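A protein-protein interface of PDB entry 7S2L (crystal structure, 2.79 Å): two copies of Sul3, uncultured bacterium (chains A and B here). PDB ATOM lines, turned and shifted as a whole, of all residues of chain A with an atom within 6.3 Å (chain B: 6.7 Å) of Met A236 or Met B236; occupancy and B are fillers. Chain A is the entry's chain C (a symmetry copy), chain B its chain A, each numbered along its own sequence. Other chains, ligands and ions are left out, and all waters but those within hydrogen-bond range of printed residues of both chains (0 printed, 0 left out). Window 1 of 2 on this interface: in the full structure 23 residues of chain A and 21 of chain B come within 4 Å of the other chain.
Among the printed residues, merely in contact across the chains: Ala A229 with Leu B232 (3.7 Å), Leu A232 with Ala B229 (3.9 Å), Ala A233 with Met B236 (3.7 Å), Ala A233 with Ala B257 (3.6 Å), Met A236 with Met B236 (3.9 Å) and Ala A257 with Ala B233 (3.6 Å).
Of the printed residues of chain B, Ala A233 touches Met B236 (3.7 Å) and Ala B257 (3.6 Å). Met A236 touches just one residue of chain B: Met B236 (3.9 Å). Lys A241 touches none of the printed residues of chain B. Of the printed residues of chain B, Ala A257 touches Ala B233. Printed residues of chain A within 4 Å of Ala B229: Leu A232 (3.9 Å). Printed residues of chain A within 4 Å of Ala B233: Ala A257. Printed residues of chain A within 4 Å of Met B236: Ala A233 and Met A236. Leu B246 touches none of the printed residues of chain A. The nearest residue of chain B that does not touch Met A236 is Ala B233 (5.0 Å).
Hydrophobic or aromatic side chains of chain A that line the printed part of chain B: Ala A229, Leu A232, Ala A233, Met A236 and Ala A257. Printed residues of chain B that touch a printed residue of chain A: Ala B229, Leu B232, Ala B233, Met B236 and Ala B257. Hydrophobic or aromatic side chains of chain B within 4 Å of the printed part of chain A: Ala B229, Leu B232, Ala B233 and Met B236.
Ala A229 touches Leu B232, and with the chains exchanged Leu A232 touches Ala B229. Ala A233 touches Met B236, but with the chains exchanged Met A236 does not touch Ala B233 (5.0 Å). Ala A233 touches Ala B257, and with the chains exchanged Ala A257 touches Ala B233. Met B236 touches its own counterpart, Met A236. Of the 6 pairs that touch across the chains among the printed residues, 5 have their exchanged pair printed and touching as well.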
ATOM      1  N   ALA A 229       8.441   8.115  -1.337  1.00  0.00           N
ATOM      2  CA  ALA A 229       7.622   7.289  -0.451  1.00  0.00           C
ATOM      3  C   ALA A 229       6.124   7.469  -0.669  1.00  0.00           C
ATOM      4  O   ALA A 229       5.436   6.469  -0.950  1.00  0.00           O
ATOM      5  CB  ALA A 229       8.020   7.554   1.004  1.00  0.00           C
ATOM      6  N   THR A 231       4.204   8.438  -2.980  1.00  0.00           N
ATOM      7  CA  THR A 231       3.771   7.804  -4.214  1.00  0.00           C
ATOM      8  C   THR A 231       3.819   6.289  -4.082  1.00  0.00           C
ATOM      9  O   THR A 231       2.809   5.608  -4.293  1.00  0.00           O
ATOM     10  CB  THR A 231       4.638   8.281  -5.373  1.00  0.00           C
ATOM     11  OG1 THR A 231       4.251   9.614  -5.725  1.00  0.00           O
ATOM     12  CG2 THR A 231       4.452   7.379  -6.576  1.00  0.00           C
ATOM     13  N   LEU A 232       4.978   5.746  -3.683  1.00  0.00           N
ATOM     14  CA  LEU A 232       5.147   4.292  -3.626  1.00  0.00           C
ATOM     15  C   LEU A 232       4.158   3.652  -2.661  1.00  0.00           C
ATOM     16  O   LEU A 232       3.620   2.573  -2.938  1.00  0.00           O
ATOM     17  CB  LEU A 232       6.580   3.942  -3.229  1.00  0.00           C
ATOM     18  CG  LEU A 232       6.962   2.478  -3.453  1.00  0.00           C
ATOM     19  CD1 LEU A 232       7.190   2.206  -4.920  1.00  0.00           C
ATOM     20  CD2 LEU A 232       8.206   2.103  -2.647  1.00  0.00           C
ATOM     21  N   ALA A 233       3.899   4.305  -1.526  1.00  0.00           N
ATOM     22  CA  ALA A 233       2.885   3.805  -0.605  1.00  0.00           C
ATOM     23  C   ALA A 233       1.541   3.619  -1.303  1.00  0.00           C
ATOM     24  O   ALA A 233       0.861   2.606  -1.098  1.00  0.00           O
ATOM     25  CB  ALA A 233       2.743   4.752   0.585  1.00  0.00           C
ATOM     26  N   ALA A 234       1.149   4.579  -2.148  1.00  0.00           N
ATOM     27  CA  ALA A 234      -0.134   4.475  -2.837  1.00  0.00           C
ATOM     28  C   ALA A 234      -0.087   3.436  -3.947  1.00  0.00           C
ATOM     29  O   ALA A 234      -1.058   2.699  -4.160  1.00  0.00           O
ATOM     30  CB  ALA A 234      -0.544   5.835  -3.399  1.00  0.00           C
ATOM     31  N   GLU A 235       1.024   3.367  -4.676  1.00  0.00           N
ATOM     32  CA  GLU A 235       1.121   2.383  -5.746  1.00  0.00           C
ATOM     33  C   GLU A 235       1.025   0.964  -5.197  1.00  0.00           C
ATOM     34  O   GLU A 235       0.372   0.107  -5.800  1.00  0.00           O
ATOM     35  CB  GLU A 235       2.415   2.591  -6.523  1.00  0.00           C
ATOM     36  CG  GLU A 235       2.559   4.004  -7.030  1.00  0.00           C
ATOM     37  CD  GLU A 235       3.827   4.223  -7.823  1.00  0.00           C
ATOM     38  OE1 GLU A 235       4.850   3.583  -7.498  1.00  0.00           O
ATOM     39  OE2 GLU A 235       3.803   5.047  -8.767  1.00  0.00           O
ATOM     40  N   MET A 236       1.651   0.699  -4.043  1.00  0.00           N
ATOM     41  CA  MET A 236       1.570  -0.642  -3.470  1.00  0.00           C
ATOM     42  C   MET A 236       0.137  -0.988  -3.106  1.00  0.00           C
ATOM     43  O   MET A 236      -0.311  -2.124  -3.311  1.00  0.00           O
ATOM     44  CB  MET A 236       2.468  -0.771  -2.235  1.00  0.00           C
ATOM     45  CG  MET A 236       3.956  -0.616  -2.492  1.00  0.00           C
ATOM     46  SD  MET A 236       4.698  -1.914  -3.499  1.00  0.00           S
ATOM     47  CE  MET A 236       3.705  -3.342  -3.081  1.00  0.00           C
ATOM     48  N   TYR A 237      -0.591  -0.018  -2.553  1.00  0.00           N
ATOM     49  CA  TYR A 237      -1.989  -0.237  -2.213  1.00  0.00           C
ATOM     50  C   TYR A 237      -2.772  -0.698  -3.434  1.00  0.00           C
ATOM     51  O   TYR A 237      -3.475  -1.718  -3.388  1.00  0.00           O
ATOM     52  CB  TYR A 237      -2.584   1.043  -1.630  1.00  0.00           C
ATOM     53  CG  TYR A 237      -4.028   0.910  -1.229  1.00  0.00           C
ATOM     54  CD1 TYR A 237      -4.372   0.344  -0.017  1.00  0.00           C
ATOM     55  CD2 TYR A 237      -5.051   1.359  -2.056  1.00  0.00           C
ATOM     56  CE1 TYR A 237      -5.690   0.214   0.365  1.00  0.00           C
ATOM     57  CE2 TYR A 237      -6.378   1.234  -1.683  1.00  0.00           C
ATOM     58  CZ  TYR A 237      -6.689   0.663  -0.465  1.00  0.00           C
ATOM     59  OH  TYR A 237      -8.001   0.527  -0.060  1.00  0.00           O
ATOM     60  N   ALA A 238      -2.631   0.032  -4.549  1.00  0.00           N
ATOM     61  CA  ALA A 238      -3.334  -0.317  -5.777  1.00  0.00           C
ATOM     62  C   ALA A 238      -2.923  -1.686  -6.299  1.00  0.00           C
ATOM     63  O   ALA A 238      -3.756  -2.410  -6.859  1.00  0.00           O
ATOM     64  CB  ALA A 238      -3.087   0.747  -6.842  1.00  0.00           C
ATOM     65  N   TYR A 239      -1.650  -2.058  -6.136  1.00  0.00           N
ATOM     66  CA  TYR A 239      -1.212  -3.385  -6.558  1.00  0.00           C
ATOM     67  C   TYR A 239      -1.946  -4.473  -5.781  1.00  0.00           C
ATOM     68  O   TYR A 239      -2.458  -5.432  -6.369  1.00  0.00           O
ATOM     69  CB  TYR A 239       0.303  -3.524  -6.389  1.00  0.00           C
ATOM     70  CG  TYR A 239       0.771  -4.959  -6.238  1.00  0.00           C
ATOM     71  CD1 TYR A 239       0.786  -5.823  -7.328  1.00  0.00           C
ATOM     72  CD2 TYR A 239       1.190  -5.450  -5.005  1.00  0.00           C
ATOM     73  CE1 TYR A 239       1.211  -7.142  -7.195  1.00  0.00           C
ATOM     74  CE2 TYR A 239       1.614  -6.768  -4.862  1.00  0.00           C
ATOM     75  CZ  TYR A 239       1.624  -7.607  -5.961  1.00  0.00           C
ATOM     76  OH  TYR A 239       2.042  -8.914  -5.834  1.00  0.00           O
ATOM     77  N   LYS A 240      -2.023  -4.337  -4.451  1.00  0.00           N
ATOM     78  CA  LYS A 240      -2.685  -5.375  -3.665  1.00  0.00           C
ATOM     79  C   LYS A 240      -4.187  -5.384  -3.904  1.00  0.00           C
ATOM     80  O   LYS A 240      -4.826  -6.438  -3.800  1.00  0.00           O
ATOM     81  CB  LYS A 240      -2.380  -5.212  -2.171  1.00  0.00           C
ATOM     82  CG  LYS A 240      -0.897  -5.086  -1.830  1.00  0.00           C
ATOM     83  CD  LYS A 240      -0.462  -6.040  -0.731  1.00  0.00           C
ATOM     84  CE  LYS A 240      -0.119  -7.431  -1.263  1.00  0.00           C
ATOM     85  NZ  LYS A 240       0.387  -8.333  -0.165  1.00  0.00           N
ATOM     86  N   LYS A 241      -4.767  -4.233  -4.234  1.00  0.00           N
ATOM     87  CA  LYS A 241      -6.185  -4.181  -4.566  1.00  0.00           C
ATOM     88  C   LYS A 241      -6.485  -4.665  -5.980  1.00  0.00           C
ATOM     89  O   LYS A 241      -7.659  -4.702  -6.367  1.00  0.00           O
ATOM     90  CB  LYS A 241      -6.726  -2.765  -4.368  1.00  0.00           C
ATOM     91  CG  LYS A 241      -6.720  -2.303  -2.914  1.00  0.00           C
ATOM     92  CD  LYS A 241      -7.510  -3.278  -2.040  1.00  0.00           C
ATOM     93  CE  LYS A 241      -8.881  -2.726  -1.635  1.00  0.00           C
ATOM     94  NZ  LYS A 241      -8.845  -1.350  -1.070  1.00  0.00           N
ATOM     95  N   LEU A 246      -0.128   0.116 -13.803  1.00  0.00           N
ATOM     96  CA  LEU A 246       0.291   1.236 -12.972  1.00  0.00           C
ATOM     97  C   LEU A 246       1.181   2.142 -13.808  1.00  0.00           C
ATOM     98  O   LEU A 246       2.191   1.690 -14.356  1.00  0.00           O
ATOM     99  CB  LEU A 246       1.019   0.748 -11.717  1.00  0.00           C
ATOM    100  CG  LEU A 246       0.133   0.105 -10.644  1.00  0.00           C
ATOM    101  CD1 LEU A 246       0.948  -0.869  -9.817  1.00  0.00           C
ATOM    102  CD2 LEU A 246      -0.507   1.140  -9.747  1.00  0.00           C
ATOM    103  N   LEU A 254       9.263   1.344  -7.955  1.00  0.00           N
ATOM    104  CA  LEU A 254       8.103   0.474  -8.049  1.00  0.00           C
ATOM    105  C   LEU A 254       8.574  -0.967  -8.163  1.00  0.00           C
ATOM    106  O   LEU A 254       8.454  -1.726  -7.199  1.00  0.00           O
ATOM    107  CB  LEU A 254       7.222   0.878  -9.234  1.00  0.00           C
ATOM    108  CG  LEU A 254       5.805   0.297  -9.269  1.00  0.00           C
ATOM    109  CD1 LEU A 254       5.075   0.494  -7.942  1.00  0.00           C
ATOM    110  CD2 LEU A 254       4.986   0.870 -10.412  1.00  0.00           C
ATOM    111  N   ALA A 257       9.838  -2.591  -5.173  1.00  0.00           N
ATOM    112  CA  ALA A 257       8.831  -2.746  -4.136  1.00  0.00           C
ATOM    113  C   ALA A 257       7.869  -3.891  -4.447  1.00  0.00           C
ATOM    114  O   ALA A 257       7.316  -4.492  -3.518  1.00  0.00           O
ATOM    115  CB  ALA A 257       8.075  -1.434  -3.938  1.00  0.00           C
ATOM    116  N   LEU A 258       7.659  -4.226  -5.725  1.00  0.00           N
ATOM    117  CA  LEU A 258       6.849  -5.412  -5.995  1.00  0.00           C
ATOM    118  C   LEU A 258       7.655  -6.702  -5.859  1.00  0.00           C
ATOM    119  O   LEU A 258       7.083  -7.750  -5.536  1.00  0.00           O
ATOM    120  CB  LEU A 258       6.185  -5.343  -7.377  1.00  0.00           C
ATOM    121  CG  LEU A 258       5.198  -4.193  -7.633  1.00  0.00           C
ATOM    122  CD1 LEU A 258       5.906  -2.964  -8.151  1.00  0.00           C
ATOM    123  CD2 LEU A 258       4.052  -4.585  -8.572  1.00  0.00           C
ATOM    124  N   SER A 261       7.306  -7.491  -2.267  1.00  0.00           N
ATOM    125  CA  SER A 261       5.963  -7.941  -1.917  1.00  0.00           C
ATOM    126  C   SER A 261       5.633  -9.300  -2.510  1.00  0.00           C
ATOM    127  O   SER A 261       4.681  -9.944  -2.059  1.00  0.00           O
ATOM    128  CB  SER A 261       4.908  -6.935  -2.363  1.00  0.00           C
ATOM    129  OG  SER A 261       3.614  -7.504  -2.231  1.00  0.00           O
ATOM    130  N   ALA B 229      13.159   1.965  -1.513  1.00  0.00           N
ATOM    131  CA  ALA B 229      11.951   1.331  -2.029  1.00  0.00           C
ATOM    132  C   ALA B 229      11.763  -0.084  -1.490  1.00  0.00           C
ATOM    133  O   ALA B 229      10.680  -0.371  -0.953  1.00  0.00           O
ATOM    134  CB  ALA B 229      11.956   1.381  -3.561  1.00  0.00           C
ATOM    135  N   THR B 231      13.001  -1.279   1.234  1.00  0.00           N
ATOM    136  CA  THR B 231      12.747  -1.036   2.652  1.00  0.00           C
ATOM    137  C   THR B 231      11.283  -0.683   2.897  1.00  0.00           C
ATOM    138  O   THR B 231      10.613  -1.319   3.718  1.00  0.00           O
ATOM    139  CB  THR B 231      13.654   0.083   3.166  1.00  0.00           C
ATOM    140  OG1 THR B 231      14.985  -0.415   3.334  1.00  0.00           O
ATOM    141  CG2 THR B 231      13.154   0.615   4.492  1.00  0.00           C
ATOM    142  N   LEU B 232      10.770   0.339   2.197  1.00  0.00           N
ATOM    143  CA  LEU B 232       9.382   0.751   2.400  1.00  0.00           C
ATOM    144  C   LEU B 232       8.416  -0.386   2.103  1.00  0.00           C
ATOM    145  O   LEU B 232       7.375  -0.510   2.761  1.00  0.00           O
ATOM    146  CB  LEU B 232       9.054   1.965   1.529  1.00  0.00           C
ATOM    147  CG  LEU B 232       9.727   3.274   1.953  1.00  0.00           C
ATOM    148  CD1 LEU B 232       9.750   4.252   0.807  1.00  0.00           C
ATOM    149  CD2 LEU B 232       9.037   3.895   3.162  1.00  0.00           C
ATOM    150  N   ALA B 233       8.742  -1.222   1.119  1.00  0.00           N
ATOM    151  CA  ALA B 233       7.906  -2.380   0.842  1.00  0.00           C
ATOM    152  C   ALA B 233       7.830  -3.296   2.055  1.00  0.00           C
ATOM    153  O   ALA B 233       6.751  -3.796   2.396  1.00  0.00           O
ATOM    154  CB  ALA B 233       8.444  -3.136  -0.374  1.00  0.00           C
ATOM    155  N   ALA B 234       8.962  -3.503   2.735  1.00  0.00           N
ATOM    156  CA  ALA B 234       8.999  -4.422   3.869  1.00  0.00           C
ATOM    157  C   ALA B 234       8.333  -3.819   5.100  1.00  0.00           C
ATOM    158  O   ALA B 234       7.510  -4.472   5.755  1.00  0.00           O
ATOM    159  CB  ALA B 234      10.445  -4.815   4.172  1.00  0.00           C
ATOM    160  N   GLU B 235       8.679  -2.572   5.428  1.00  0.00           N
ATOM    161  CA  GLU B 235       8.082  -1.919   6.585  1.00  0.00           C
ATOM    162  C   GLU B 235       6.569  -1.841   6.454  1.00  0.00           C
ATOM    163  O   GLU B 235       5.840  -2.016   7.438  1.00  0.00           O
ATOM    164  CB  GLU B 235       8.681  -0.529   6.756  1.00  0.00           C
ATOM    165  CG  GLU B 235      10.026  -0.549   7.412  1.00  0.00           C
ATOM    166  CD  GLU B 235      10.884   0.646   7.066  1.00  0.00           C
ATOM    167  OE1 GLU B 235      10.425   1.517   6.302  1.00  0.00           O
ATOM    168  OE2 GLU B 235      12.020   0.727   7.578  1.00  0.00           O
ATOM    169  N   MET B 236       6.071  -1.584   5.246  1.00  0.00           N
ATOM    170  CA  MET B 236       4.627  -1.575   5.053  1.00  0.00           C
ATOM    171  C   MET B 236       4.050  -2.960   5.298  1.00  0.00           C
ATOM    172  O   MET B 236       2.995  -3.102   5.928  1.00  0.00           O
ATOM    173  CB  MET B 236       4.287  -1.083   3.648  1.00  0.00           C
ATOM    174  CG  MET B 236       4.380   0.422   3.479  1.00  0.00           C
ATOM    175  SD  MET B 236       3.596   0.953   1.929  1.00  0.00           S
ATOM    176  CE  MET B 236       5.004   1.086   0.822  1.00  0.00           C
ATOM    177  N   TYR B 237       4.746  -3.996   4.834  1.00  0.00           N
ATOM    178  CA  TYR B 237       4.264  -5.356   5.028  1.00  0.00           C
ATOM    179  C   TYR B 237       4.157  -5.686   6.515  1.00  0.00           C
ATOM    180  O   TYR B 237       3.136  -6.213   6.977  1.00  0.00           O
ATOM    181  CB  TYR B 237       5.191  -6.329   4.305  1.00  0.00           C
ATOM    182  CG  TYR B 237       4.893  -7.779   4.573  1.00  0.00           C
ATOM    183  CD1 TYR B 237       3.992  -8.475   3.784  1.00  0.00           C
ATOM    184  CD2 TYR B 237       5.517  -8.457   5.617  1.00  0.00           C
ATOM    185  CE1 TYR B 237       3.714  -9.808   4.022  1.00  0.00           C
ATOM    186  CE2 TYR B 237       5.247  -9.784   5.862  1.00  0.00           C
ATOM    187  CZ  TYR B 237       4.347 -10.457   5.061  1.00  0.00           C
ATOM    188  OH  TYR B 237       4.070 -11.785   5.301  1.00  0.00           O
ATOM    189  N   ALA B 238       5.203  -5.364   7.283  1.00  0.00           N
ATOM    190  CA  ALA B 238       5.177  -5.615   8.719  1.00  0.00           C
ATOM    191  C   ALA B 238       4.057  -4.840   9.397  1.00  0.00           C
ATOM    192  O   ALA B 238       3.418  -5.344  10.331  1.00  0.00           O
ATOM    193  CB  ALA B 238       6.523  -5.249   9.339  1.00  0.00           C
ATOM    194  N   TYR B 239       3.807  -3.609   8.942  1.00  0.00           N
ATOM    195  CA  TYR B 239       2.737  -2.806   9.522  1.00  0.00           C
ATOM    196  C   TYR B 239       1.386  -3.484   9.334  1.00  0.00           C
ATOM    197  O   TYR B 239       0.624  -3.656  10.294  1.00  0.00           O
ATOM    198  CB  TYR B 239       2.726  -1.410   8.894  1.00  0.00           C
ATOM    199  CG  TYR B 239       1.380  -0.713   8.964  1.00  0.00           C
ATOM    200  CD1 TYR B 239       0.969  -0.065  10.128  1.00  0.00           C
ATOM    201  CD2 TYR B 239       0.521  -0.703   7.869  1.00  0.00           C
ATOM    202  CE1 TYR B 239      -0.259   0.578  10.197  1.00  0.00           C
ATOM    203  CE2 TYR B 239      -0.710  -0.067   7.930  1.00  0.00           C
ATOM    204  CZ  TYR B 239      -1.092   0.573   9.094  1.00  0.00           C
ATOM    205  OH  TYR B 239      -2.313   1.206   9.153  1.00  0.00           O
ATOM    206  N   LYS B 240       1.075  -3.883   8.097  1.00  0.00           N
ATOM    207  CA  LYS B 240      -0.232  -4.464   7.820  1.00  0.00           C
ATOM    208  C   LYS B 240      -0.437  -5.767   8.581  1.00  0.00           C
ATOM    209  O   LYS B 240      -1.574  -6.120   8.913  1.00  0.00           O
ATOM    210  CB  LYS B 240      -0.405  -4.681   6.312  1.00  0.00           C
ATOM    211  CG  LYS B 240      -1.831  -5.041   5.891  1.00  0.00           C
ATOM    212  CD  LYS B 240      -1.899  -6.460   5.325  1.00  0.00           C
ATOM    213  CE  LYS B 240      -3.331  -6.982   5.275  1.00  0.00           C
ATOM    214  NZ  LYS B 240      -4.046  -6.762   6.568  1.00  0.00           N
ATOM    215  N   LYS B 241       0.647  -6.484   8.881  1.00  0.00           N
ATOM    216  CA  LYS B 241       0.555  -7.745   9.599  1.00  0.00           C
ATOM    217  C   LYS B 241       0.552  -7.573  11.111  1.00  0.00           C
ATOM    218  O   LYS B 241       0.368  -8.561  11.831  1.00  0.00           O
ATOM    219  CB  LYS B 241       1.699  -8.674   9.181  1.00  0.00           C
ATOM    220  CG  LYS B 241       1.405  -9.461   7.911  1.00  0.00           C
ATOM    221  CD  LYS B 241       2.383 -10.609   7.739  1.00  0.00           C
ATOM    222  CE  LYS B 241       1.861 -11.895   8.359  1.00  0.00           C
ATOM    223  NZ  LYS B 241       2.771 -13.039   8.071  1.00  0.00           N
ATOM    224  N   LEU B 246       8.706  -0.495  14.548  1.00  0.00           N
ATOM    225  CA  LEU B 246       9.474  -0.555  13.314  1.00  0.00           C
ATOM    226  C   LEU B 246      10.709   0.311  13.494  1.00  0.00           C
ATOM    227  O   LEU B 246      10.598   1.484  13.864  1.00  0.00           O
ATOM    228  CB  LEU B 246       8.629  -0.101  12.116  1.00  0.00           C
ATOM    229  CG  LEU B 246       7.465  -1.019  11.698  1.00  0.00           C
ATOM    230  CD1 LEU B 246       6.550  -0.354  10.690  1.00  0.00           C
ATOM    231  CD2 LEU B 246       7.988  -2.341  11.144  1.00  0.00           C
ATOM    232  N   LEU B 254       9.037   6.436   6.060  1.00  0.00           N
ATOM    233  CA  LEU B 254       8.179   5.448   6.699  1.00  0.00           C
ATOM    234  C   LEU B 254       6.896   6.091   7.200  1.00  0.00           C
ATOM    235  O   LEU B 254       5.804   5.541   7.014  1.00  0.00           O
ATOM    236  CB  LEU B 254       8.921   4.757   7.840  1.00  0.00           C
ATOM    237  CG  LEU B 254       8.083   3.725   8.604  1.00  0.00           C
ATOM    238  CD1 LEU B 254       7.481   2.698   7.646  1.00  0.00           C
ATOM    239  CD2 LEU B 254       8.888   3.053   9.722  1.00  0.00           C
ATOM    240  N   ALA B 257       4.679   6.395   4.327  1.00  0.00           N
ATOM    241  CA  ALA B 257       4.104   5.113   3.940  1.00  0.00           C
ATOM    242  C   ALA B 257       2.948   4.736   4.858  1.00  0.00           C
ATOM    243  O   ALA B 257       1.885   4.310   4.386  1.00  0.00           O
ATOM    244  CB  ALA B 257       5.183   4.032   3.939  1.00  0.00           C
ATOM    245  N   LEU B 258       3.121   4.928   6.169  1.00  0.00           N
ATOM    246  CA  LEU B 258       2.071   4.565   7.117  1.00  0.00           C
ATOM    247  C   LEU B 258       0.885   5.516   7.024  1.00  0.00           C
ATOM    248  O   LEU B 258      -0.274   5.082   7.072  1.00  0.00           O
ATOM    249  CB  LEU B 258       2.629   4.548   8.537  1.00  0.00           C
ATOM    250  CG  LEU B 258       3.179   3.236   9.101  1.00  0.00           C
ATOM    251  CD1 LEU B 258       3.935   2.408   8.062  1.00  0.00           C
ATOM    252  CD2 LEU B 258       4.064   3.546  10.292  1.00  0.00           C
ATOM    253  N   SER B 261      -1.073   4.571   4.017  1.00  0.00           N
ATOM    254  CA  SER B 261      -1.709   3.260   4.140  1.00  0.00           C
ATOM    255  C   SER B 261      -2.888   3.299   5.102  1.00  0.00           C
ATOM    256  O   SER B 261      -3.918   2.655   4.858  1.00  0.00           O
ATOM    257  CB  SER B 261      -0.686   2.222   4.594  1.00  0.00           C
ATOM    258  OG  SER B 261       0.584   2.483   4.023  1.00  0.00           O
